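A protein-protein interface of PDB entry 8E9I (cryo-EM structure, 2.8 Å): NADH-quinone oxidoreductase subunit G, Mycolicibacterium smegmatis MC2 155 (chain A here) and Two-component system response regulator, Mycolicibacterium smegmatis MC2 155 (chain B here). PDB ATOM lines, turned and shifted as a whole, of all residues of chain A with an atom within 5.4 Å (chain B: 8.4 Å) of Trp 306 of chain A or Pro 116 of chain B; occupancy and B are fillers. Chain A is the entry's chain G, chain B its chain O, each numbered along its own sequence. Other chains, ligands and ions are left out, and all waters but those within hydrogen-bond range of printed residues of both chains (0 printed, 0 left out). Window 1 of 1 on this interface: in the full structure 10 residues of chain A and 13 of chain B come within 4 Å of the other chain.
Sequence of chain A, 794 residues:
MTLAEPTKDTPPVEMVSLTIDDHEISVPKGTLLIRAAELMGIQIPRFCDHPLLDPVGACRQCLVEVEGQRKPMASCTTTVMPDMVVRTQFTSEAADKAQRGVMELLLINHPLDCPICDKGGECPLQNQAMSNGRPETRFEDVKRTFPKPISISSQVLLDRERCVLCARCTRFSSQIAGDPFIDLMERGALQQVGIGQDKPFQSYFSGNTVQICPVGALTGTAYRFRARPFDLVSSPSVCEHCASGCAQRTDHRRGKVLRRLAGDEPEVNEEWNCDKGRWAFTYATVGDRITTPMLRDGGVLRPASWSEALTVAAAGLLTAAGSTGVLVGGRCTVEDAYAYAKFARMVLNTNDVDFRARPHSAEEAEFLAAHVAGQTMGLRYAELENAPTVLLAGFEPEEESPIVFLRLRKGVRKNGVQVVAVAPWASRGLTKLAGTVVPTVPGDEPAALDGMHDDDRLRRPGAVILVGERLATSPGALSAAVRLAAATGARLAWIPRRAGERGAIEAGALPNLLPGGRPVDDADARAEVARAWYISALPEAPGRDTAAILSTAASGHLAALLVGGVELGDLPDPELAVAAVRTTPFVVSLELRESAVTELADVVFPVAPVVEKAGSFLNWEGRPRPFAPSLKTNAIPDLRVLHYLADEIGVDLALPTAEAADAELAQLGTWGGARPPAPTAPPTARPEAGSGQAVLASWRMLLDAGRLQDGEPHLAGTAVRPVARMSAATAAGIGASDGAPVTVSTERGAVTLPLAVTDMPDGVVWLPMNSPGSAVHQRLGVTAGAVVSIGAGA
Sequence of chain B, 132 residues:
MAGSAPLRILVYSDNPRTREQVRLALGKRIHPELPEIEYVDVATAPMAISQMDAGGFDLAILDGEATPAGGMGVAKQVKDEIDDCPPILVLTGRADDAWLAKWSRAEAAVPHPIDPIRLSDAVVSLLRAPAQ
The side-chain carboxylate (OD1) of Asp 115 of chain B lies close to the backbone NH (N) of Ile 117 of chain B, 3.5 Å away. The backbone NH (N) of Ser 307 of chain A lies close to the side-chain hydroxyl (OG) of Ser 305 of chain A (3.5 Å). The backbone NH of Glu 308 of chain A sits at hydrogen-bond distance from the side-chain hydroxyl of Ser 305 of chain A (2.8 Å). O of Ser 307 of chain A sits at hydrogen-bond distance from OG1 of Thr 311 of chain A, 2.8 Å away.
Printed residues of chain B that touch a printed residue of chain A: Gln 21, Leu 24, Ala 25, Gly 27, Arg 29, Ile 30, Pro 113, Ile 114, Asp 115, Pro 116, Ile 117 and Ser 120. Along chain B the printed residues that touch a printed residue of chain A span positions 21 to 120. Among the printed residues, no Asp or Glu carboxylate lies within 4 Å of a Lys or Arg side-chain nitrogen of the other chain.
Among the printed residues, pairs that only touch across the chains: Ser 305 of chain A with Leu 24 of chain B (3.1 Å), Ser 305 of chain A with Gly 27 of chain B (3.0 Å), Trp 306 of chain A with Pro 116 of chain B (3.3 Å), Ser 307 of chain A with Gly 27 of chain B (3.6 Å), Ser 307 of chain A with Arg 29 of chain B (3.9 Å), Ser 307 of chain A with Ile 30 of chain B (3.2 Å), Ser 307 of chain A with Ser 120 of chain B (3.7 Å), Asn 634 of chain A with Pro 113 of chain B (3.5 Å), Asn 634 of chain A with Ile 114 of chain B (3.3 Å), Asn 634 of chain A with Pro 116 of chain B (3.8 Å), Ile 636 of chain A with Asp 115 of chain B (3.8 Å) and Ile 636 of chain A with Ile 117 of chain B (3.5 Å).
NE2 of Gln 21 of chain B sits close to ND2 of Asn 634 of chain A, 3.1 Å away. N of Trp 306 of chain A sits at hydrogen-bond distance from O of Leu 24 of chain B, 3.0 Å away. OG of Ser 307 of chain A sits at hydrogen-bond distance from O of Ala 25 of chain B (3.3 Å).
Trp 306 of chain A touches just these residues of chain B: Leu 24 (3.0 Å) and Pro 116 (3.3 Å). Pro 116 of chain B touches just these residues of chain A: Trp 306 (3.3 Å) and Asn 634 (3.8 Å). Of the printed residues of chain A, Gly 27 of chain B touches Ser 305 and Ser 307. Of the printed residues of chain A, Ile 117 of chain B touches Ile 636. Of the printed residues of chain A, Arg 29 of chain B touches Ser 307. Printed residues of chain A within 4 Å of Ile 114 of chain B: Asn 634 (3.3 Å). The nearest printed residue of chain B that does not touch Asn 634 of chain A is Asp 115 of chain B (4.7 Å).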
ATOM      1  N   PRO A 293      16.048  30.535  23.757  1.00  0.00           N
ATOM      2  CA  PRO A 293      17.425  30.097  23.537  1.00  0.00           C
ATOM      3  C   PRO A 293      18.361  31.292  23.520  1.00  0.00           C
ATOM      4  O   PRO A 293      18.042  32.350  22.977  1.00  0.00           O
ATOM      5  CB  PRO A 293      17.363  29.397  22.178  1.00  0.00           C
ATOM      6  CG  PRO A 293      15.965  28.953  22.055  1.00  0.00           C
ATOM      7  CD  PRO A 293      15.135  29.998  22.738  1.00  0.00           C
ATOM      8  N   ALA A 304      18.166  34.378  21.273  1.00  0.00           N
ATOM      9  CA  ALA A 304      18.303  33.837  19.933  1.00  0.00           C
ATOM     10  C   ALA A 304      17.100  32.972  19.603  1.00  0.00           C
ATOM     11  O   ALA A 304      16.387  32.495  20.486  1.00  0.00           O
ATOM     12  CB  ALA A 304      19.585  33.013  19.790  1.00  0.00           C
ATOM     13  N   SER A 305      16.886  32.777  18.308  1.00  0.00           N
ATOM     14  CA  SER A 305      15.833  31.892  17.849  1.00  0.00           C
ATOM     15  C   SER A 305      16.174  30.446  18.184  1.00  0.00           C
ATOM     16  O   SER A 305      17.299  30.116  18.566  1.00  0.00           O
ATOM     17  CB  SER A 305      15.643  32.030  16.343  1.00  0.00           C
ATOM     18  OG  SER A 305      16.764  31.505  15.654  1.00  0.00           O
ATOM     19  N   TRP A 306      15.176  29.576  18.051  1.00  0.00           N
ATOM     20  CA  TRP A 306      15.440  28.148  18.158  1.00  0.00           C
ATOM     21  C   TRP A 306      16.207  27.641  16.946  1.00  0.00           C
ATOM     22  O   TRP A 306      17.113  26.811  17.079  1.00  0.00           O
ATOM     23  CB  TRP A 306      14.132  27.380  18.330  1.00  0.00           C
ATOM     24  CG  TRP A 306      13.631  27.414  19.724  1.00  0.00           C
ATOM     25  CD1 TRP A 306      12.676  28.234  20.232  1.00  0.00           C
ATOM     26  CD2 TRP A 306      14.075  26.592  20.808  1.00  0.00           C
ATOM     27  NE1 TRP A 306      12.489  27.972  21.565  1.00  0.00           N
ATOM     28  CE2 TRP A 306      13.337  26.966  21.942  1.00  0.00           C
ATOM     29  CE3 TRP A 306      15.022  25.576  20.926  1.00  0.00           C
ATOM     30  CZ2 TRP A 306      13.521  26.364  23.179  1.00  0.00           C
ATOM     31  CZ3 TRP A 306      15.198  24.976  22.154  1.00  0.00           C
ATOM     32  CH2 TRP A 306      14.453  25.373  23.264  1.00  0.00           C
ATOM     33  N   SER A 307      15.865  28.129  15.755  1.00  0.00           N
ATOM     34  CA  SER A 307      16.559  27.678  14.556  1.00  0.00           C
ATOM     35  C   SER A 307      18.041  28.016  14.624  1.00  0.00           C
ATOM     36  O   SER A 307      18.898  27.139  14.459  1.00  0.00           O
ATOM     37  CB  SER A 307      15.922  28.305  13.320  1.00  0.00           C
ATOM     38  OG  SER A 307      14.615  27.802  13.121  1.00  0.00           O
ATOM     39  N   GLU A 308      18.363  29.283  14.883  1.00  0.00           N
ATOM     40  CA  GLU A 308      19.762  29.689  14.947  1.00  0.00           C
ATOM     41  C   GLU A 308      20.485  28.966  16.074  1.00  0.00           C
ATOM     42  O   GLU A 308      21.619  28.502  15.904  1.00  0.00           O
ATOM     43  CB  GLU A 308      19.859  31.202  15.132  1.00  0.00           C
ATOM     44  N   ALA A 309      19.843  28.868  17.238  1.00  0.00           N
ATOM     45  CA  ALA A 309      20.490  28.229  18.376  1.00  0.00           C
ATOM     46  C   ALA A 309      20.815  26.776  18.075  1.00  0.00           C
ATOM     47  O   ALA A 309      21.918  26.307  18.373  1.00  0.00           O
ATOM     48  CB  ALA A 309      19.602  28.334  19.612  1.00  0.00           C
ATOM     49  N   LEU A 310      19.869  26.044  17.493  1.00  0.00           N
ATOM     50  CA  LEU A 310      20.127  24.647  17.168  1.00  0.00           C
ATOM     51  C   LEU A 310      21.203  24.534  16.101  1.00  0.00           C
ATOM     52  O   LEU A 310      22.050  23.638  16.154  1.00  0.00           O
ATOM     53  CB  LEU A 310      18.841  23.963  16.711  1.00  0.00           C
ATOM     54  CG  LEU A 310      17.842  23.693  17.832  1.00  0.00           C
ATOM     55  CD1 LEU A 310      16.525  23.218  17.255  1.00  0.00           C
ATOM     56  CD2 LEU A 310      18.399  22.680  18.814  1.00  0.00           C
ATOM     57  N   THR A 311      21.185  25.435  15.120  1.00  0.00           N
ATOM     58  CA  THR A 311      22.245  25.444  14.120  1.00  0.00           C
ATOM     59  C   THR A 311      23.609  25.535  14.788  1.00  0.00           C
ATOM     60  O   THR A 311      24.508  24.730  14.515  1.00  0.00           O
ATOM     61  CB  THR A 311      22.038  26.616  13.158  1.00  0.00           C
ATOM     62  OG1 THR A 311      20.783  26.473  12.486  1.00  0.00           O
ATOM     63  CG2 THR A 311      23.158  26.680  12.133  1.00  0.00           C
ATOM     64  N   PHE A 605      19.785  26.609  26.115  1.00  0.00           N
ATOM     65  CA  PHE A 605      18.445  26.221  25.712  1.00  0.00           C
ATOM     66  C   PHE A 605      17.521  26.225  26.916  1.00  0.00           C
ATOM     67  O   PHE A 605      17.891  25.679  27.962  1.00  0.00           O
ATOM     68  CB  PHE A 605      18.460  24.832  25.081  1.00  0.00           C
ATOM     69  CG  PHE A 605      19.195  24.769  23.782  1.00  0.00           C
ATOM     70  CD1 PHE A 605      18.592  25.185  22.611  1.00  0.00           C
ATOM     71  CD2 PHE A 605      20.494  24.303  23.730  1.00  0.00           C
ATOM     72  CE1 PHE A 605      19.266  25.134  21.416  1.00  0.00           C
ATOM     73  CE2 PHE A 605      21.175  24.248  22.537  1.00  0.00           C
ATOM     74  CZ  PHE A 605      20.561  24.665  21.378  1.00  0.00           C
ATOM     75  N   PRO A 606      16.338  26.825  26.830  1.00  0.00           N
ATOM     76  CA  PRO A 606      15.391  26.730  27.942  1.00  0.00           C
ATOM     77  C   PRO A 606      14.616  25.424  27.912  1.00  0.00           C
ATOM     78  O   PRO A 606      14.076  25.019  26.881  1.00  0.00           O
ATOM     79  CB  PRO A 606      14.467  27.927  27.718  1.00  0.00           C
ATOM     80  CG  PRO A 606      14.469  28.110  26.254  1.00  0.00           C
ATOM     81  CD  PRO A 606      15.844  27.726  25.776  1.00  0.00           C
ATOM     82  N   ASN A 634       4.365  26.890  26.142  1.00  0.00           N
ATOM     83  CA  ASN A 634       5.189  26.713  24.956  1.00  0.00           C
ATOM     84  C   ASN A 634       6.509  26.024  25.270  1.00  0.00           C
ATOM     85  O   ASN A 634       7.178  25.547  24.348  1.00  0.00           O
ATOM     86  CB  ASN A 634       5.467  28.065  24.306  1.00  0.00           C
ATOM     87  CG  ASN A 634       6.045  29.069  25.283  1.00  0.00           C
ATOM     88  OD1 ASN A 634       7.043  28.798  25.950  1.00  0.00           O
ATOM     89  ND2 ASN A 634       5.424  30.238  25.369  1.00  0.00           N
ATOM     90  N   ILE A 636       9.446  23.410  26.334  1.00  0.00           N
ATOM     91  CA  ILE A 636       9.646  22.014  25.958  1.00  0.00           C
ATOM     92  C   ILE A 636      10.583  21.360  26.966  1.00  0.00           C
ATOM     93  O   ILE A 636      11.404  22.052  27.581  1.00  0.00           O
ATOM     94  CB  ILE A 636      10.199  21.896  24.530  1.00  0.00           C
ATOM     95  CG1 ILE A 636      11.431  22.777  24.361  1.00  0.00           C
ATOM     96  CG2 ILE A 636       9.141  22.291  23.516  1.00  0.00           C
ATOM     97  CD1 ILE A 636      11.986  22.751  22.969  1.00  0.00           C
ATOM     98  N   VAL A 641      14.302  18.989  23.383  1.00  0.00           N
ATOM     99  CA  VAL A 641      15.461  19.812  23.059  1.00  0.00           C
ATOM    100  C   VAL A 641      16.589  18.938  22.531  1.00  0.00           C
ATOM    101  O   VAL A 641      17.157  19.201  21.466  1.00  0.00           O
ATOM    102  CB  VAL A 641      15.904  20.623  24.288  1.00  0.00           C
ATOM    103  CG1 VAL A 641      17.183  21.377  23.987  1.00  0.00           C
ATOM    104  CG2 VAL A 641      14.814  21.585  24.700  1.00  0.00           C
ATOM    105  N   GLU B  20       6.363  37.692  18.755  1.00  0.00           N
ATOM    106  CA  GLU B  20       7.731  37.412  19.176  1.00  0.00           C
ATOM    107  C   GLU B  20       7.976  35.912  19.253  1.00  0.00           C
ATOM    108  O   GLU B  20       9.054  35.432  18.898  1.00  0.00           O
ATOM    109  CB  GLU B  20       8.010  38.074  20.522  1.00  0.00           C
ATOM    110  N   GLN B  21       6.983  35.159  19.714  1.00  0.00           N
ATOM    111  CA  GLN B  21       7.119  33.712  19.805  1.00  0.00           C
ATOM    112  C   GLN B  21       7.292  33.094  18.424  1.00  0.00           C
ATOM    113  O   GLN B  21       8.120  32.197  18.228  1.00  0.00           O
ATOM    114  CB  GLN B  21       5.895  33.140  20.515  1.00  0.00           C
ATOM    115  CG  GLN B  21       6.029  31.700  20.936  1.00  0.00           C
ATOM    116  CD  GLN B  21       6.608  31.553  22.320  1.00  0.00           C
ATOM    117  OE1 GLN B  21       6.685  32.516  23.078  1.00  0.00           O
ATOM    118  NE2 GLN B  21       7.021  30.340  22.661  1.00  0.00           N
ATOM    119  N   VAL B  22       6.519  33.568  17.447  1.00  0.00           N
ATOM    120  CA  VAL B  22       6.659  33.070  16.080  1.00  0.00           C
ATOM    121  C   VAL B  22       8.033  33.424  15.528  1.00  0.00           C
ATOM    122  O   VAL B  22       8.707  32.596  14.907  1.00  0.00           O
ATOM    123  CB  VAL B  22       5.541  33.632  15.186  1.00  0.00           C
ATOM    124  CG1 VAL B  22       5.825  33.310  13.732  1.00  0.00           C
ATOM    125  CG2 VAL B  22       4.200  33.071  15.609  1.00  0.00           C
ATOM    126  N   ARG B  23       8.461  34.664  15.735  1.00  0.00           N
ATOM    127  CA  ARG B  23       9.785  35.073  15.292  1.00  0.00           C
ATOM    128  C   ARG B  23      10.899  34.305  15.988  1.00  0.00           C
ATOM    129  O   ARG B  23      11.991  34.191  15.424  1.00  0.00           O
ATOM    130  CB  ARG B  23       9.963  36.572  15.523  1.00  0.00           C
ATOM    131  CG  ARG B  23      11.389  37.066  15.322  1.00  0.00           C
ATOM    132  CD  ARG B  23      11.448  38.570  15.104  1.00  0.00           C
ATOM    133  NE  ARG B  23      10.526  39.290  15.976  1.00  0.00           N
ATOM    134  CZ  ARG B  23       9.309  39.684  15.623  1.00  0.00           C
ATOM    135  NH1 ARG B  23       8.822  39.439  14.418  1.00  0.00           N
ATOM    136  NH2 ARG B  23       8.560  40.342  16.503  1.00  0.00           N
ATOM    137  N   LEU B  24      10.663  33.784  17.189  1.00  0.00           N
ATOM    138  CA  LEU B  24      11.668  32.982  17.872  1.00  0.00           C
ATOM    139  C   LEU B  24      11.705  31.579  17.292  1.00  0.00           C
ATOM    140  O   LEU B  24      12.781  31.056  16.992  1.00  0.00           O
ATOM    141  CB  LEU B  24      11.387  32.916  19.371  1.00  0.00           C
ATOM    142  CG  LEU B  24      11.654  34.169  20.202  1.00  0.00           C
ATOM    143  CD1 LEU B  24      11.528  33.829  21.670  1.00  0.00           C
ATOM    144  CD2 LEU B  24      13.022  34.765  19.910  1.00  0.00           C
ATOM    145  N   ALA B  25      10.539  30.958  17.135  1.00  0.00           N
ATOM    146  CA  ALA B  25      10.500  29.627  16.543  1.00  0.00           C
ATOM    147  C   ALA B  25      11.210  29.614  15.199  1.00  0.00           C
ATOM    148  O   ALA B  25      11.916  28.657  14.867  1.00  0.00           O
ATOM    149  CB  ALA B  25       9.054  29.163  16.388  1.00  0.00           C
ATOM    150  N   LEU B  26      11.038  30.669  14.413  1.00  0.00           N
ATOM    151  CA  LEU B  26      11.686  30.801  13.119  1.00  0.00           C
ATOM    152  C   LEU B  26      12.817  31.814  13.210  1.00  0.00           C
ATOM    153  O   LEU B  26      12.575  33.018  13.326  1.00  0.00           O
ATOM    154  CB  LEU B  26      10.693  31.259  12.054  1.00  0.00           C
ATOM    155  CG  LEU B  26       9.299  30.647  12.076  1.00  0.00           C
ATOM    156  CD1 LEU B  26       8.435  31.361  11.068  1.00  0.00           C
ATOM    157  CD2 LEU B  26       9.339  29.163  11.795  1.00  0.00           C
ATOM    158  N   GLY B  27      14.053  31.334  13.115  1.00  0.00           N
ATOM    159  CA  GLY B  27      15.208  32.202  13.137  1.00  0.00           C
ATOM    160  C   GLY B  27      15.326  32.961  11.828  1.00  0.00           C
ATOM    161  O   GLY B  27      14.533  32.770  10.904  1.00  0.00           O
ATOM    162  N   LYS B  28      16.336  33.831  11.777  1.00  0.00           N
ATOM    163  CA  LYS B  28      16.627  34.528  10.530  1.00  0.00           C
ATOM    164  C   LYS B  28      16.856  33.532   9.404  1.00  0.00           C
ATOM    165  O   LYS B  28      16.595  33.831   8.235  1.00  0.00           O
ATOM    166  CB  LYS B  28      17.846  35.433  10.707  1.00  0.00           C
ATOM    167  N   ARG B  29      17.336  32.333   9.740  1.00  0.00           N
ATOM    168  CA  ARG B  29      17.590  31.279   8.761  1.00  0.00           C
ATOM    169  C   ARG B  29      17.138  29.948   9.365  1.00  0.00           C
ATOM    170  O   ARG B  29      17.895  29.265  10.054  1.00  0.00           O
ATOM    171  CB  ARG B  29      19.061  31.247   8.360  1.00  0.00           C
ATOM    172  CG  ARG B  29      19.418  30.122   7.418  1.00  0.00           C
ATOM    173  CD  ARG B  29      20.875  30.195   7.008  1.00  0.00           C
ATOM    174  NE  ARG B  29      21.119  31.258   6.039  1.00  0.00           N
ATOM    175  CZ  ARG B  29      21.019  31.115   4.724  1.00  0.00           C
ATOM    176  NH1 ARG B  29      20.647  29.970   4.177  1.00  0.00           N
ATOM    177  NH2 ARG B  29      21.297  32.151   3.938  1.00  0.00           N
ATOM    178  N   ILE B  30      15.887  29.579   9.102  1.00  0.00           N
ATOM    179  CA  ILE B  30      15.384  28.282   9.537  1.00  0.00           C
ATOM    180  C   ILE B  30      15.873  27.215   8.570  1.00  0.00           C
ATOM    181  O   ILE B  30      15.830  27.401   7.347  1.00  0.00           O
ATOM    182  CB  ILE B  30      13.850  28.294   9.620  1.00  0.00           C
ATOM    183  CG1 ILE B  30      13.226  28.526   8.244  1.00  0.00           C
ATOM    184  CG2 ILE B  30      13.381  29.378  10.563  1.00  0.00           C
ATOM    185  CD1 ILE B  30      11.739  28.320   8.224  1.00  0.00           C
ATOM    186  N   HIS B  31      16.331  26.089   9.105  1.00  0.00           N
ATOM    187  CA  HIS B  31      16.788  25.027   8.220  1.00  0.00           C
ATOM    188  C   HIS B  31      17.920  25.547   7.340  1.00  0.00           C
ATOM    189  O   HIS B  31      17.705  25.801   6.149  1.00  0.00           O
ATOM    190  CB  HIS B  31      15.637  24.509   7.359  1.00  0.00           C
ATOM    191  N   VAL B 110      -1.200  25.194  13.621  1.00  0.00           N
ATOM    192  CA  VAL B 110      -0.343  24.909  14.764  1.00  0.00           C
ATOM    193  C   VAL B 110      -1.057  25.379  16.025  1.00  0.00           C
ATOM    194  O   VAL B 110      -1.283  26.579  16.194  1.00  0.00           O
ATOM    195  CB  VAL B 110       1.029  25.590  14.632  1.00  0.00           C
ATOM    196  CG1 VAL B 110       1.841  25.400  15.905  1.00  0.00           C
ATOM    197  CG2 VAL B 110       1.773  25.029  13.442  1.00  0.00           C
ATOM    198  N   PRO B 111      -1.435  24.488  16.938  1.00  0.00           N
ATOM    199  CA  PRO B 111      -2.181  24.932  18.121  1.00  0.00           C
ATOM    200  C   PRO B 111      -1.334  25.786  19.049  1.00  0.00           C
ATOM    201  O   PRO B 111      -0.121  25.601  19.162  1.00  0.00           O
ATOM    202  CB  PRO B 111      -2.586  23.616  18.798  1.00  0.00           C
ATOM    203  CG  PRO B 111      -2.438  22.574  17.745  1.00  0.00           C
ATOM    204  CD  PRO B 111      -1.296  23.025  16.910  1.00  0.00           C
ATOM    205  N   PRO B 113      -0.197  26.722  22.853  1.00  0.00           N
ATOM    206  CA  PRO B 113       0.891  27.692  22.710  1.00  0.00           C
ATOM    207  C   PRO B 113       1.855  27.275  21.615  1.00  0.00           C
ATOM    208  O   PRO B 113       2.028  26.081  21.392  1.00  0.00           O
ATOM    209  CB  PRO B 113       1.569  27.653  24.072  1.00  0.00           C
ATOM    210  CG  PRO B 113       1.335  26.276  24.547  1.00  0.00           C
ATOM    211  CD  PRO B 113      -0.024  25.893  24.056  1.00  0.00           C
ATOM    212  N   ILE B 114       2.478  28.240  20.947  1.00  0.00           N
ATOM    213  CA  ILE B 114       3.330  27.933  19.806  1.00  0.00           C
ATOM    214  C   ILE B 114       4.456  27.012  20.249  1.00  0.00           C
ATOM    215  O   ILE B 114       5.316  27.404  21.045  1.00  0.00           O
ATOM    216  CB  ILE B 114       3.901  29.209  19.170  1.00  0.00           C
ATOM    217  CG1 ILE B 114       2.779  30.133  18.705  1.00  0.00           C
ATOM    218  CG2 ILE B 114       4.790  28.853  18.003  1.00  0.00           C
ATOM    219  CD1 ILE B 114       3.056  31.584  18.971  1.00  0.00           C
ATOM    220  N   ASP B 115       4.463  25.794  19.731  1.00  0.00           N
ATOM    221  CA  ASP B 115       5.576  24.888  19.955  1.00  0.00           C
ATOM    222  C   ASP B 115       6.680  25.229  18.961  1.00  0.00           C
ATOM    223  O   ASP B 115       6.450  25.140  17.749  1.00  0.00           O
ATOM    224  CB  ASP B 115       5.120  23.445  19.790  1.00  0.00           C
ATOM    225  CG  ASP B 115       6.203  22.442  20.131  1.00  0.00           C
ATOM    226  OD1 ASP B 115       7.395  22.810  20.134  1.00  0.00           O
ATOM    227  OD2 ASP B 115       5.858  21.275  20.397  1.00  0.00           O
ATOM    228  N   PRO B 116       7.877  25.614  19.409  1.00  0.00           N
ATOM    229  CA  PRO B 116       8.855  26.154  18.451  1.00  0.00           C
ATOM    230  C   PRO B 116       9.205  25.191  17.336  1.00  0.00           C
ATOM    231  O   PRO B 116       9.181  25.568  16.160  1.00  0.00           O
ATOM    232  CB  PRO B 116      10.069  26.462  19.335  1.00  0.00           C
ATOM    233  CG  PRO B 116       9.551  26.510  20.716  1.00  0.00           C
ATOM    234  CD  PRO B 116       8.438  25.532  20.764  1.00  0.00           C
ATOM    235  N   ILE B 117       9.533  23.947  17.672  1.00  0.00           N
ATOM    236  CA  ILE B 117       9.975  23.009  16.648  1.00  0.00           C
ATOM    237  C   ILE B 117       8.812  22.621  15.747  1.00  0.00           C
ATOM    238  O   ILE B 117       8.975  22.464  14.535  1.00  0.00           O
ATOM    239  CB  ILE B 117      10.637  21.779  17.286  1.00  0.00           C
ATOM    240  CG1 ILE B 117      11.924  22.201  17.999  1.00  0.00           C
ATOM    241  CG2 ILE B 117      10.917  20.743  16.226  1.00  0.00           C
ATOM    242  CD1 ILE B 117      11.763  22.411  19.483  1.00  0.00           C
ATOM    243  N   ARG B 118       7.620  22.451  16.321  1.00  0.00           N
ATOM    244  CA  ARG B 118       6.467  22.136  15.486  1.00  0.00           C
ATOM    245  C   ARG B 118       6.198  23.247  14.483  1.00  0.00           C
ATOM    246  O   ARG B 118       5.941  22.981  13.304  1.00  0.00           O
ATOM    247  CB  ARG B 118       5.230  21.903  16.346  1.00  0.00           C
ATOM    248  CG  ARG B 118       4.004  21.518  15.533  1.00  0.00           C
ATOM    249  CD  ARG B 118       2.815  21.180  16.415  1.00  0.00           C
ATOM    250  NE  ARG B 118       1.614  20.950  15.621  1.00  0.00           N
ATOM    251  CZ  ARG B 118       0.512  20.371  16.075  1.00  0.00           C
ATOM    252  NH1 ARG B 118       0.422  19.935  17.320  1.00  0.00           N
ATOM    253  NH2 ARG B 118      -0.527  20.226  15.261  1.00  0.00           N
ATOM    254  N   LEU B 119       6.247  24.502  14.935  1.00  0.00           N
ATOM    255  CA  LEU B 119       6.006  25.614  14.024  1.00  0.00           C
ATOM    256  C   LEU B 119       7.096  25.701  12.969  1.00  0.00           C
ATOM    257  O   LEU B 119       6.811  25.957  11.795  1.00  0.00           O
ATOM    258  CB  LEU B 119       5.911  26.924  14.801  1.00  0.00           C
ATOM    259  CG  LEU B 119       5.655  28.161  13.938  1.00  0.00           C
ATOM    260  CD1 LEU B 119       4.343  28.023  13.202  1.00  0.00           C
ATOM    261  CD2 LEU B 119       5.652  29.414  14.775  1.00  0.00           C
ATOM    262  N   SER B 120       8.349  25.490  13.366  1.00  0.00           N
ATOM    263  CA  SER B 120       9.437  25.536  12.397  1.00  0.00           C
ATOM    264  C   SER B 120       9.280  24.442  11.353  1.00  0.00           C
ATOM    265  O   SER B 120       9.483  24.674  10.156  1.00  0.00           O
ATOM    266  CB  SER B 120      10.779  25.406  13.114  1.00  0.00           C
ATOM    267  OG  SER B 120      11.852  25.453  12.193  1.00  0.00           O
ATOM    268  N   ASP B 121       8.925  23.234  11.785  1.00  0.00           N
ATOM    269  CA  ASP B 121       8.753  22.133  10.847  1.00  0.00           C
ATOM    270  C   ASP B 121       7.583  22.399   9.913  1.00  0.00           C
ATOM    271  O   ASP B 121       7.672  22.153   8.705  1.00  0.00           O
ATOM    272  CB  ASP B 121       8.552  20.824  11.608  1.00  0.00           C
ATOM    273  N   ALA B 122       6.473  22.904  10.451  1.00  0.00           N
ATOM    274  CA  ALA B 122       5.347  23.253   9.597  1.00  0.00           C
ATOM    275  C   ALA B 122       5.762  24.274   8.550  1.00  0.00           C
ATOM    276  O   ALA B 122       5.457  24.123   7.361  1.00  0.00           O
ATOM    277  CB  ALA B 122       4.194  23.793  10.439  1.00  0.00           C
ATOM    278  N   VAL B 123       6.470  25.322   8.971  1.00  0.00           N
ATOM    279  CA  VAL B 123       6.876  26.363   8.034  1.00  0.00           C
ATOM    280  C   VAL B 123       7.792  25.785   6.966  1.00  0.00           C
ATOM    281  O   VAL B 123       7.625  26.046   5.770  1.00  0.00           O
ATOM    282  CB  VAL B 123       7.553  27.523   8.783  1.00  0.00           C
ATOM    283  CG1 VAL B 123       8.249  28.441   7.803  1.00  0.00           C
ATOM    284  CG2 VAL B 123       6.529  28.285   9.606  1.00  0.00           C
